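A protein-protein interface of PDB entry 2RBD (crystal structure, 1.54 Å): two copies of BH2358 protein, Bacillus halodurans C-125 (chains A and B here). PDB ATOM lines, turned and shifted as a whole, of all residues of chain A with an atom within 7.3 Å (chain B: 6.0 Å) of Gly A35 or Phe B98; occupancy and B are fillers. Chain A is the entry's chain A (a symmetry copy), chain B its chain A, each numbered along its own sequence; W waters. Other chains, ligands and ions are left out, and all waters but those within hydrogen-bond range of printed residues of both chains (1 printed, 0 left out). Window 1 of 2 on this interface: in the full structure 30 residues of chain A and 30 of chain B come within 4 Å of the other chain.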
ATOM      1  N   ASN A  29     -21.548  27.996  14.473  1.00  0.00           N
ATOM      2  CA  ASN A  29     -20.529  26.954  14.564  1.00  0.00           C
ATOM      3  C   ASN A  29     -20.751  26.073  15.807  1.00  0.00           C
ATOM      4  O   ASN A  29     -20.637  24.851  15.718  1.00  0.00           O
ATOM      5  CB  ASN A  29     -19.110  27.514  14.584  1.00  0.00           C
ATOM      6  CG  ASN A  29     -18.544  27.804  13.195  1.00  0.00           C
ATOM      7  OD1 ASN A  29     -19.240  27.634  12.191  1.00  0.00           O
ATOM      8  ND2 ASN A  29     -17.284  28.237  13.138  1.00  0.00           N
ATOM      9  N   ASN A  30     -21.018  26.670  16.955  1.00  0.00           N
ATOM     10  CA  ASN A  30     -21.223  25.882  18.163  1.00  0.00           C
ATOM     11  C   ASN A  30     -22.362  24.901  17.994  1.00  0.00           C
ATOM     12  O   ASN A  30     -22.304  23.750  18.428  1.00  0.00           O
ATOM     13  CB  ASN A  30     -21.532  26.824  19.338  1.00  0.00           C
ATOM     14  CG  ASN A  30     -20.334  27.604  19.827  1.00  0.00           C
ATOM     15  OD1 ASN A  30     -19.178  27.227  19.622  1.00  0.00           O
ATOM     16  ND2 ASN A  30     -20.627  28.675  20.569  1.00  0.00           N
ATOM     17  N   GLY A  31     -23.433  25.359  17.360  1.00  0.00           N
ATOM     18  CA  GLY A  31     -24.592  24.497  17.108  1.00  0.00           C
ATOM     19  C   GLY A  31     -24.299  23.392  16.123  1.00  0.00           C
ATOM     20  O   GLY A  31     -24.734  22.232  16.277  1.00  0.00           O
ATOM     21  N   LEU A  32     -23.569  23.741  15.094  1.00  0.00           N
ATOM     22  CA  LEU A  32     -23.202  22.734  14.072  1.00  0.00           C
ATOM     23  C   LEU A  32     -22.211  21.701  14.597  1.00  0.00           C
ATOM     24  O   LEU A  32     -22.354  20.532  14.319  1.00  0.00           O
ATOM     25  CB  LEU A  32     -22.681  23.394  12.797  1.00  0.00           C
ATOM     26  CG  LEU A  32     -23.675  24.233  11.976  1.00  0.00           C
ATOM     27  CD1 LEU A  32     -22.922  24.808  10.765  1.00  0.00           C
ATOM     28  CD2 LEU A  32     -24.873  23.372  11.498  1.00  0.00           C
ATOM     29  N   ILE A  33     -21.256  22.116  15.427  1.00  0.00           N
ATOM     30  CA  ILE A  33     -20.381  21.176  16.090  1.00  0.00           C
ATOM     31  C   ILE A  33     -21.207  20.144  16.885  1.00  0.00           C
ATOM     32  O   ILE A  33     -20.960  18.949  16.815  1.00  0.00           O
ATOM     33  CB  ILE A  33     -19.362  21.906  16.959  1.00  0.00           C
ATOM     34  CG1 ILE A  33     -18.329  22.642  16.060  1.00  0.00           C
ATOM     35  CG2 ILE A  33     -18.624  20.921  17.849  1.00  0.00           C
ATOM     36  CD1 ILE A  33     -17.455  23.640  16.818  1.00  0.00           C
ATOM     37  N   ASN A  34     -22.182  20.629  17.645  1.00  0.00           N
ATOM     38  CA  ASN A  34     -23.018  19.745  18.439  1.00  0.00           C
ATOM     39  C   ASN A  34     -23.825  18.794  17.563  1.00  0.00           C
ATOM     40  O   ASN A  34     -23.848  17.598  17.806  1.00  0.00           O
ATOM     41  CB  ASN A  34     -23.928  20.595  19.325  1.00  0.00           C
ATOM     42  CG  ASN A  34     -24.942  19.757  20.088  1.00  0.00           C
ATOM     43  OD1 ASN A  34     -24.568  18.867  20.793  1.00  0.00           O
ATOM     44  ND2 ASN A  34     -26.208  20.047  19.930  1.00  0.00           N
ATOM     45  N   GLY A  35     -24.467  19.315  16.525  1.00  0.00           N
ATOM     46  CA  GLY A  35     -25.239  18.456  15.612  1.00  0.00           C
ATOM     47  C   GLY A  35     -24.397  17.443  14.876  1.00  0.00           C
ATOM     48  O   GLY A  35     -24.791  16.292  14.731  1.00  0.00           O
ATOM     49  N   TYR A  36     -23.227  17.867  14.427  1.00  0.00           N
ATOM     50  CA  TYR A  36     -22.345  16.979  13.704  1.00  0.00           C
ATOM     51  C   TYR A  36     -21.752  15.902  14.637  1.00  0.00           C
ATOM     52  O   TYR A  36     -21.534  14.793  14.215  1.00  0.00           O
ATOM     53  CB  TYR A  36     -21.218  17.746  13.012  1.00  0.00           C
ATOM     54  CG  TYR A  36     -21.634  18.593  11.844  1.00  0.00           C
ATOM     55  CD1 TYR A  36     -22.958  18.915  11.594  1.00  0.00           C
ATOM     56  CD2 TYR A  36     -20.673  19.181  11.059  1.00  0.00           C
ATOM     57  CE1 TYR A  36     -23.311  19.744  10.506  1.00  0.00           C
ATOM     58  CE2 TYR A  36     -21.021  20.001   9.981  1.00  0.00           C
ATOM     59  CZ  TYR A  36     -22.314  20.276   9.726  1.00  0.00           C
ATOM     60  OH  TYR A  36     -22.619  21.119   8.671  1.00  0.00           O
ATOM     61  N   ARG A  37     -21.474  16.246  15.890  1.00  0.00           N
ATOM     62  CA  ARG A  37     -21.070  15.225  16.857  1.00  0.00           C
ATOM     63  C   ARG A  37     -22.179  14.180  17.040  1.00  0.00           C
ATOM     64  O   ARG A  37     -21.914  12.976  17.182  1.00  0.00           O
ATOM     65  CB  ARG A  37     -20.682  15.905  18.153  1.00  0.00           C
ATOM     66  CG  ARG A  37     -19.297  16.531  18.080  1.00  0.00           C
ATOM     67  CD  ARG A  37     -19.025  17.336  19.334  1.00  0.00           C
ATOM     68  NE  ARG A  37     -17.603  17.640  19.468  1.00  0.00           N
ATOM     69  CZ  ARG A  37     -17.134  18.498  20.365  1.00  0.00           C
ATOM     70  NH1 ARG A  37     -17.935  19.227  21.114  1.00  0.00           N
ATOM     71  NH2 ARG A  37     -15.837  18.649  20.504  1.00  0.00           N
ATOM     72  N   SER A  38     -23.432  14.625  16.977  1.00  0.00           N
ATOM     73  CA  SER A  38     -24.532  13.648  17.000  1.00  0.00           C
ATOM     74  C   SER A  38     -24.529  12.842  15.704  1.00  0.00           C
ATOM     75  O   SER A  38     -24.561  11.614  15.740  1.00  0.00           O
ATOM     76  CB  SER A  38     -25.872  14.323  17.186  1.00  0.00           C
ATOM     77  OG  SER A  38     -26.889  13.345  17.283  1.00  0.00           O
ATOM     78  N   PHE A  39     -24.370  13.513  14.555  1.00  0.00           N
ATOM     79  CA  PHE A  39     -24.298  12.799  13.273  1.00  0.00           C
ATOM     80  C   PHE A  39     -23.194  11.744  13.220  1.00  0.00           C
ATOM     81  O   PHE A  39     -23.394  10.715  12.615  1.00  0.00           O
ATOM     82  CB  PHE A  39     -24.108  13.769  12.128  1.00  0.00           C
ATOM     83  CG  PHE A  39     -25.340  14.568  11.748  1.00  0.00           C
ATOM     84  CD1 PHE A  39     -26.633  14.186  12.081  1.00  0.00           C
ATOM     85  CD2 PHE A  39     -25.174  15.685  10.965  1.00  0.00           C
ATOM     86  CE1 PHE A  39     -27.735  14.953  11.667  1.00  0.00           C
ATOM     87  CE2 PHE A  39     -26.254  16.457  10.556  1.00  0.00           C
ATOM     88  CZ  PHE A  39     -27.528  16.088  10.925  1.00  0.00           C
ATOM     89  N   ILE A  40     -22.054  11.974  13.859  1.00  0.00           N
ATOM     90  CA  ILE A  40     -21.009  10.944  13.908  1.00  0.00           C
ATOM     91  C   ILE A  40     -21.581   9.638  14.457  1.00  0.00           C
ATOM     92  O   ILE A  40     -21.306   8.571  13.942  1.00  0.00           O
ATOM     93  CB  ILE A  40     -19.780  11.416  14.762  1.00  0.00           C
ATOM     94  CG1 ILE A  40     -18.812  12.203  13.875  1.00  0.00           C
ATOM     95  CG2 ILE A  40     -19.033  10.243  15.424  1.00  0.00           C
ATOM     96  CD1 ILE A  40     -18.065  13.263  14.643  1.00  0.00           C
ATOM     97  N   ASN A  41     -22.399   9.743  15.495  1.00  0.00           N
ATOM     98  CA  ASN A  41     -23.037   8.580  16.102  1.00  0.00           C
ATOM     99  C   ASN A  41     -24.111   7.911  15.241  1.00  0.00           C
ATOM    100  O   ASN A  41     -24.405   6.732  15.440  1.00  0.00           O
ATOM    101  CB  ASN A  41     -23.593   8.959  17.462  1.00  0.00           C
ATOM    102  CG  ASN A  41     -22.486   9.143  18.508  1.00  0.00           C
ATOM    103  OD1 ASN A  41     -21.521   8.397  18.491  1.00  0.00           O
ATOM    104  ND2 ASN A  41     -22.643  10.078  19.416  1.00  0.00           N
ATOM    105  N   HIS A  42     -24.704   8.647  14.308  1.00  0.00           N
ATOM    106  CA  HIS A  42     -25.744   8.151  13.407  1.00  0.00           C
ATOM    107  C   HIS A  42     -25.192   7.607  12.107  1.00  0.00           C
ATOM    108  O   HIS A  42     -25.919   7.027  11.358  1.00  0.00           O
ATOM    109  CB  HIS A  42     -26.719   9.284  13.011  1.00  0.00           C
ATOM    110  CG  HIS A  42     -27.672   9.684  14.084  1.00  0.00           C
ATOM    111  ND1 HIS A  42     -29.004   9.375  14.051  1.00  0.00           N
ATOM    112  CD2 HIS A  42     -27.490  10.389  15.220  1.00  0.00           C
ATOM    113  CE1 HIS A  42     -29.610   9.879  15.115  1.00  0.00           C
ATOM    114  NE2 HIS A  42     -28.710  10.506  15.849  1.00  0.00           N
ATOM    115  N   ILE A  52     -17.096  14.493   8.427  1.00  0.00           N
ATOM    116  CA  ILE A  52     -17.778  15.148   9.550  1.00  0.00           C
ATOM    117  C   ILE A  52     -16.729  15.527  10.572  1.00  0.00           C
ATOM    118  O   ILE A  52     -16.732  16.642  11.098  1.00  0.00           O
ATOM    119  CB  ILE A  52     -18.851  14.248  10.209  1.00  0.00           C
ATOM    120  CG1 ILE A  52     -19.957  13.814   9.253  1.00  0.00           C
ATOM    121  CG2 ILE A  52     -19.415  14.976  11.468  1.00  0.00           C
ATOM    122  CD1 ILE A  52     -20.872  12.742   9.836  1.00  0.00           C
ATOM    123  N   ILE A  56     -15.890  19.326  11.912  1.00  0.00           N
ATOM    124  CA  ILE A  56     -15.843  19.698  13.335  1.00  0.00           C
ATOM    125  C   ILE A  56     -14.517  20.373  13.643  1.00  0.00           C
ATOM    126  O   ILE A  56     -14.477  21.425  14.269  1.00  0.00           O
ATOM    127  CB  ILE A  56     -16.058  18.476  14.212  1.00  0.00           C
ATOM    128  CG1 ILE A  56     -17.509  17.960  14.070  1.00  0.00           C
ATOM    129  CG2 ILE A  56     -15.743  18.804  15.688  1.00  0.00           C
ATOM    130  CD1 ILE A  56     -17.716  16.501  14.512  1.00  0.00           C
ATOM    131  N   PRO A  81     -23.165  24.155  23.223  1.00  0.00           N
ATOM    132  CA  PRO A  81     -23.485  22.826  23.757  1.00  0.00           C
ATOM    133  C   PRO A  81     -22.248  21.992  24.017  1.00  0.00           C
ATOM    134  O   PRO A  81     -21.227  22.176  23.364  1.00  0.00           O
ATOM    135  CB  PRO A  81     -24.298  22.197  22.646  1.00  0.00           C
ATOM    136  CG  PRO A  81     -24.840  23.322  21.896  1.00  0.00           C
ATOM    137  CD  PRO A  81     -23.803  24.404  21.933  1.00  0.00           C
ATOM    138  N   ARG A  84     -20.306  15.131  23.330  1.00  0.00           N
ATOM    139  CA  ARG A  84     -21.316  14.078  23.413  1.00  0.00           C
ATOM    140  C   ARG A  84     -20.656  12.739  23.652  1.00  0.00           C
ATOM    141  O   ARG A  84     -19.573  12.461  23.149  1.00  0.00           O
ATOM    142  CB  ARG A  84     -22.094  13.954  22.078  1.00  0.00           C
ATOM    143  CG  ARG A  84     -23.029  15.089  21.822  1.00  0.00           C
ATOM    144  CD  ARG A  84     -23.651  14.953  20.465  1.00  0.00           C
ATOM    145  NE  ARG A  84     -24.735  15.910  20.397  1.00  0.00           N
ATOM    146  CZ  ARG A  84     -25.984  15.615  20.667  1.00  0.00           C
ATOM    147  NH1 ARG A  84     -26.306  14.349  20.925  1.00  0.00           N
ATOM    148  NH2 ARG A  84     -26.893  16.554  20.643  1.00  0.00           N
ATOM    149  N   ALA A  96     -35.693   7.458  14.909  1.00  0.00           N
ATOM    150  CA  ALA A  96     -34.843   8.549  15.418  1.00  0.00           C
ATOM    151  C   ALA A  96     -33.541   8.688  14.653  1.00  0.00           C
ATOM    152  O   ALA A  96     -32.758   9.622  14.885  1.00  0.00           O
ATOM    153  CB  ALA A  96     -34.558   8.312  16.906  1.00  0.00           C
ATOM    154  N   PHE A  98     -30.822   9.278  11.695  1.00  0.00           N
ATOM    155  CA  PHE A  98     -30.512   9.972  10.477  1.00  0.00           C
ATOM    156  C   PHE A  98     -29.615   9.088   9.653  1.00  0.00           C
ATOM    157  O   PHE A  98     -28.654   8.516  10.140  1.00  0.00           O
ATOM    158  CB  PHE A  98     -29.832  11.318  10.757  1.00  0.00           C
ATOM    159  CG  PHE A  98     -30.768  12.321  11.408  1.00  0.00           C
ATOM    160  CD1 PHE A  98     -31.587  13.104  10.661  1.00  0.00           C
ATOM    161  CD2 PHE A  98     -30.844  12.408  12.770  1.00  0.00           C
ATOM    162  CE1 PHE A  98     -32.479  14.007  11.303  1.00  0.00           C
ATOM    163  CE2 PHE A  98     -31.742  13.285  13.385  1.00  0.00           C
ATOM    164  CZ  PHE A  98     -32.550  14.049  12.640  1.00  0.00           C
ATOM    165  N   ILE A 103     -27.721  12.937   6.072  1.00  0.00           N
ATOM    166  CA  ILE A 103     -26.659  13.600   6.838  1.00  0.00           C
ATOM    167  C   ILE A 103     -25.765  14.384   5.873  1.00  0.00           C
ATOM    168  O   ILE A 103     -25.458  15.547   6.088  1.00  0.00           O
ATOM    169  CB  ILE A 103     -25.819  12.584   7.613  1.00  0.00           C
ATOM    170  CG1 ILE A 103     -26.642  11.985   8.764  1.00  0.00           C
ATOM    171  CG2 ILE A 103     -24.549  13.247   8.211  1.00  0.00           C
ATOM    172  CD1 ILE A 103     -26.027  10.718   9.372  1.00  0.00           C
ATOM    173  N   PHE B  39     -37.054  14.596  14.403  1.00  0.00           N
ATOM    174  CA  PHE B  39     -37.114  15.446  15.598  1.00  0.00           C
ATOM    175  C   PHE B  39     -38.339  15.190  16.474  1.00  0.00           C
ATOM    176  O   PHE B  39     -38.228  15.265  17.677  1.00  0.00           O
ATOM    177  CB  PHE B  39     -37.077  16.910  15.219  1.00  0.00           C
ATOM    178  CG  PHE B  39     -35.723  17.428  14.774  1.00  0.00           C
ATOM    179  CD1 PHE B  39     -34.524  16.796  15.076  1.00  0.00           C
ATOM    180  CD2 PHE B  39     -35.674  18.628  14.106  1.00  0.00           C
ATOM    181  CE1 PHE B  39     -33.300  17.347  14.664  1.00  0.00           C
ATOM    182  CE2 PHE B  39     -34.471  19.180  13.684  1.00  0.00           C
ATOM    183  CZ  PHE B  39     -33.292  18.524  13.958  1.00  0.00           C
ATOM    184  N   HIS B  42     -37.349  12.693  18.891  1.00  0.00           N
ATOM    185  CA  HIS B  42     -36.313  13.148  19.816  1.00  0.00           C
ATOM    186  C   HIS B  42     -36.822  14.152  20.829  1.00  0.00           C
ATOM    187  O   HIS B  42     -36.119  14.477  21.737  1.00  0.00           O
ATOM    188  CB  HIS B  42     -35.167  13.857  19.058  1.00  0.00           C
ATOM    189  CG  HIS B  42     -34.262  12.942  18.308  1.00  0.00           C
ATOM    190  ND1 HIS B  42     -32.985  12.663  18.709  1.00  0.00           N
ATOM    191  CD2 HIS B  42     -34.442  12.252  17.163  1.00  0.00           C
ATOM    192  CE1 HIS B  42     -32.407  11.846  17.841  1.00  0.00           C
ATOM    193  NE2 HIS B  42     -33.274  11.578  16.884  1.00  0.00           N
ATOM    194  N   THR B  43     -38.014  14.696  20.687  1.00  0.00           N
ATOM    195  CA  THR B  43     -38.496  15.817  21.483  1.00  0.00           C
ATOM    196  C   THR B  43     -39.248  15.338  22.737  1.00  0.00           C
ATOM    197  O   THR B  43     -40.076  14.431  22.624  1.00  0.00           O
ATOM    198  CB  THR B  43     -39.509  16.668  20.623  1.00  0.00           C
ATOM    199  OG1 THR B  43     -38.856  17.181  19.437  1.00  0.00           O
ATOM    200  CG2 THR B  43     -40.101  17.820  21.430  1.00  0.00           C
ATOM    201  N   ILE B  92     -33.419   6.258  22.855  1.00  0.00           N
ATOM    202  CA  ILE B  92     -32.415   6.901  21.993  1.00  0.00           C
ATOM    203  C   ILE B  92     -31.138   7.040  22.812  1.00  0.00           C
ATOM    204  O   ILE B  92     -31.153   7.691  23.867  1.00  0.00           O
ATOM    205  CB  ILE B  92     -32.844   8.295  21.469  1.00  0.00           C
ATOM    206  CG1 ILE B  92     -34.215   8.222  20.759  1.00  0.00           C
ATOM    207  CG2 ILE B  92     -31.772   8.856  20.533  1.00  0.00           C
ATOM    208  CD1 ILE B  92     -34.882   9.604  20.463  1.00  0.00           C
ATOM    209  N   VAL B  94     -27.954   8.559  24.406  1.00  0.00           N
ATOM    210  CA  VAL B  94     -27.774   9.958  24.735  1.00  0.00           C
ATOM    211  C   VAL B  94     -26.932  10.699  23.693  1.00  0.00           C
ATOM    212  O   VAL B  94     -27.243  11.799  23.281  1.00  0.00           O
ATOM    213  CB  VAL B  94     -27.128  10.089  26.132  1.00  0.00           C
ATOM    214  CG1 VAL B  94     -26.674  11.510  26.386  1.00  0.00           C
ATOM    215  CG2 VAL B  94     -28.124   9.625  27.197  1.00  0.00           C
ATOM    216  N   ALA B  96     -26.703  10.190  20.602  1.00  0.00           N
ATOM    217  CA  ALA B  96     -27.440  10.314  19.332  1.00  0.00           C
ATOM    218  C   ALA B  96     -28.644  11.229  19.436  1.00  0.00           C
ATOM    219  O   ALA B  96     -29.312  11.526  18.434  1.00  0.00           O
ATOM    220  CB  ALA B  96     -27.877   8.919  18.866  1.00  0.00           C
ATOM    221  N   ARG B  97     -28.936  11.686  20.643  1.00  0.00           N
ATOM    222  CA  ARG B  97     -30.183  12.406  20.938  1.00  0.00           C
ATOM    223  C   ARG B  97     -30.038  13.893  20.676  1.00  0.00           C
ATOM    224  O   ARG B  97     -29.090  14.522  21.148  1.00  0.00           O
ATOM    225  CB  ARG B  97     -30.564  12.207  22.429  1.00  0.00           C
ATOM    226  CG  ARG B  97     -31.473  13.332  23.060  1.00  0.00           C
ATOM    227  CD  ARG B  97     -32.876  12.903  23.433  1.00  0.00           C
ATOM    228  NE  ARG B  97     -33.859  13.999  23.346  1.00  0.00           N
ATOM    229  CZ  ARG B  97     -34.144  14.914  24.274  1.00  0.00           C
ATOM    230  NH1 ARG B  97     -33.474  14.976  25.420  1.00  0.00           N
ATOM    231  NH2 ARG B  97     -35.078  15.844  24.019  1.00  0.00           N
ATOM    232  N   PHE B  98     -31.006  14.488  19.984  1.00  0.00           N
ATOM    233  CA  PHE B  98     -31.119  15.915  19.873  1.00  0.00           C
ATOM    234  C   PHE B  98     -32.053  16.394  20.951  1.00  0.00           C
ATOM    235  O   PHE B  98     -33.119  15.841  21.169  1.00  0.00           O
ATOM    236  CB  PHE B  98     -31.635  16.331  18.489  1.00  0.00           C
ATOM    237  CG  PHE B  98     -30.631  16.052  17.384  1.00  0.00           C
ATOM    238  CD1 PHE B  98     -29.658  16.946  17.079  1.00  0.00           C
ATOM    239  CD2 PHE B  98     -30.658  14.861  16.714  1.00  0.00           C
ATOM    240  CE1 PHE B  98     -28.710  16.640  16.064  1.00  0.00           C
ATOM    241  CE2 PHE B  98     -29.706  14.567  15.734  1.00  0.00           C
ATOM    242  CZ  PHE B  98     -28.745  15.453  15.444  1.00  0.00           C
ATOM    243  N   ASN B  99     -31.609  17.418  21.632  1.00  0.00           N
ATOM    244  CA  ASN B  99     -32.334  17.971  22.752  1.00  0.00           C
ATOM    245  C   ASN B  99     -33.213  19.132  22.331  1.00  0.00           C
ATOM    246  O   ASN B  99     -32.929  19.800  21.355  1.00  0.00           O
ATOM    247  CB  ASN B  99     -31.320  18.405  23.820  1.00  0.00           C
ATOM    248  CG  ASN B  99     -30.448  17.243  24.246  1.00  0.00           C
ATOM    249  OD1 ASN B  99     -30.965  16.285  24.815  1.00  0.00           O
ATOM    250  ND2 ASN B  99     -29.151  17.263  23.875  1.00  0.00           N
ATOM    251  N   ASP B 100     -34.203  19.438  23.162  1.00  0.00           N
ATOM    252  CA  ASP B 100     -35.249  20.388  22.785  1.00  0.00           C
ATOM    253  C   ASP B 100     -34.735  21.777  22.378  1.00  0.00           C
ATOM    254  O   ASP B 100     -35.111  22.277  21.351  1.00  0.00           O
ATOM    255  CB  ASP B 100     -36.298  20.526  23.896  1.00  0.00           C
ATOM    256  CG  ASP B 100     -37.066  19.243  24.127  1.00  0.00           C
ATOM    257  OD1 ASP B 100     -37.057  18.350  23.252  1.00  0.00           O
ATOM    258  OD2 ASP B 100     -37.677  19.107  25.186  1.00  0.00           O
ATOM    259  N   GLU B 102     -31.870  22.666  21.171  1.00  0.00           N
ATOM    260  CA  GLU B 102     -31.158  22.637  19.915  1.00  0.00           C
ATOM    261  C   GLU B 102     -32.085  22.292  18.728  1.00  0.00           C
ATOM    262  O   GLU B 102     -31.896  22.873  17.662  1.00  0.00           O
ATOM    263  CB  GLU B 102     -29.925  21.762  20.023  1.00  0.00           C
ATOM    264  CG  GLU B 102     -28.797  22.420  20.832  1.00  0.00           C
ATOM    265  CD  GLU B 102     -29.038  22.439  22.330  1.00  0.00           C
ATOM    266  OE1 GLU B 102     -29.619  21.460  22.858  1.00  0.00           O
ATOM    267  OE2 GLU B 102     -28.629  23.430  22.983  1.00  0.00           O
ATOM    268  N   ILE B 103     -33.116  21.491  18.926  1.00  0.00           N
ATOM    269  CA  ILE B 103     -34.141  21.230  17.908  1.00  0.00           C
ATOM    270  C   ILE B 103     -34.839  22.547  17.556  1.00  0.00           C
ATOM    271  O   ILE B 103     -35.007  22.892  16.397  1.00  0.00           O
ATOM    272  CB  ILE B 103     -35.169  20.215  18.406  1.00  0.00           C
ATOM    273  CG1 ILE B 103     -34.532  18.821  18.505  1.00  0.00           C
ATOM    274  CG2 ILE B 103     -36.386  20.132  17.445  1.00  0.00           C
ATOM    275  CD1 ILE B 103     -35.358  17.817  19.319  1.00  0.00           C
HETATM  276  O   HOH W   1     -27.609  14.445  24.108  1.00  0.00           O
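Hydrophobic or aromatic side chains of chain A that line the printed part of chain B: Phe A39, His A42, Pro A81, Ala A96 and Phe A98. Among the printed residues, no Asp or Glu carboxylate lies within 4 Å of a Lys or Arg side-chain nitrogen of the other chain.
Of chain B, only Phe B98 (3.9 Å) comes within 4 Å of Gly A35. Phe B98 touches four residues of chain A. Of the printed residues of chain B, Ser A38 touches Ala B96 (3.2 Å) and Phe B98 (3.4 Å). Printed residues of chain A within 4 Å of Phe B39: Phe A98 (3.9 Å). The nearest residue of chain A that does not touch Phe B98 is His A42 (4.2 Å). The nearest printed residue of chain A that does not touch Glu B102 is Gly A31 (6.0 Å).
Glu B102 touches Asn A34 (CG to ND2, 3.6 Å). CA of Gly A35 touches CE1 of Phe B98 (3.9 Å). Ser A38 touches Phe B98 (OG to CZ, 3.4 Å). Phe A39 touches Phe B98 (CE1 to CZ, 3.9 Å). Pro A81 touches Glu B102 (CG to OE2, 3.9 Å). O of Val B94 touches NH1 of Arg A84 (3.6 Å). Ile B92 touches Ala A96 (CD1 to CB, 3.8 Å). CE1 of Phe B39 touches CZ of Phe A98 (3.9 Å). Phe A98 touches Phe B98.
The backbone carbonyl oxygen of His B42 lies within hydrogen-bond range of the guanidinium group of Arg B97, at 2.8 Å. ND1 of His B42 sits at hydrogen-bond distance from N of Phe B98, 3.0 Å away. The side-chain amide oxygen of Asn B99 lies within hydrogen-bond range of the guanidinium group of Arg B97 (2.9 Å). The guanidinium group (NH2) of Arg B97 lies within salt-bridge range of the side-chain carboxylate (OD1) of Asp B100 (3.3 Å). The guanidinium group of Arg A84 lies within hydrogen-bond range of the side-chain amide oxygen of Asn A34 (3.0 Å). The backbone NH (N) of Phe A98 sits at hydrogen-bond distance from a ring nitrogen (ND1) of His A42.
Water W1 lies within hydrogen-bond range of the backbone carbonyl oxygen of Val B94 (2.8 Å), the side-chain amide nitrogen of Asn B99 (3.2 Å), the backbone carbonyl oxygen of Arg B97 (3.3 Å) and the guanidinium group of Arg A84 (3.4 Å).
Phe A39 touches Phe B98, and with the chains exchanged Phe A98 touches Phe B39. His A42 touches Ala B96, and with the chains exchanged Ala A96 touches His B42. Phe B98 touches its own counterpart, Phe A98. Positions printed for both chains: 39, 42, 96, 98 and 103. Of the 13 pairs that touch across the chains among the printed residues, 5 have their exchanged pair printed and touching as well.
O of Ala A96 lies within hydrogen-bond range of NE2 of His B42 (2.8 Å). OG of Ser A38 sits at hydrogen-bond distance from O of Ala B96 (3.2 Å). A ring nitrogen (NE2) of His A42 lies within hydrogen-bond range of the backbone carbonyl oxygen (O) of Ala B96 (2.8 Å). The guanidinium group (NH1) of Arg A84 is in hydrogen-bond range of the backbone carbonyl oxygen (O) of Arg B97 (2.8 Å).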
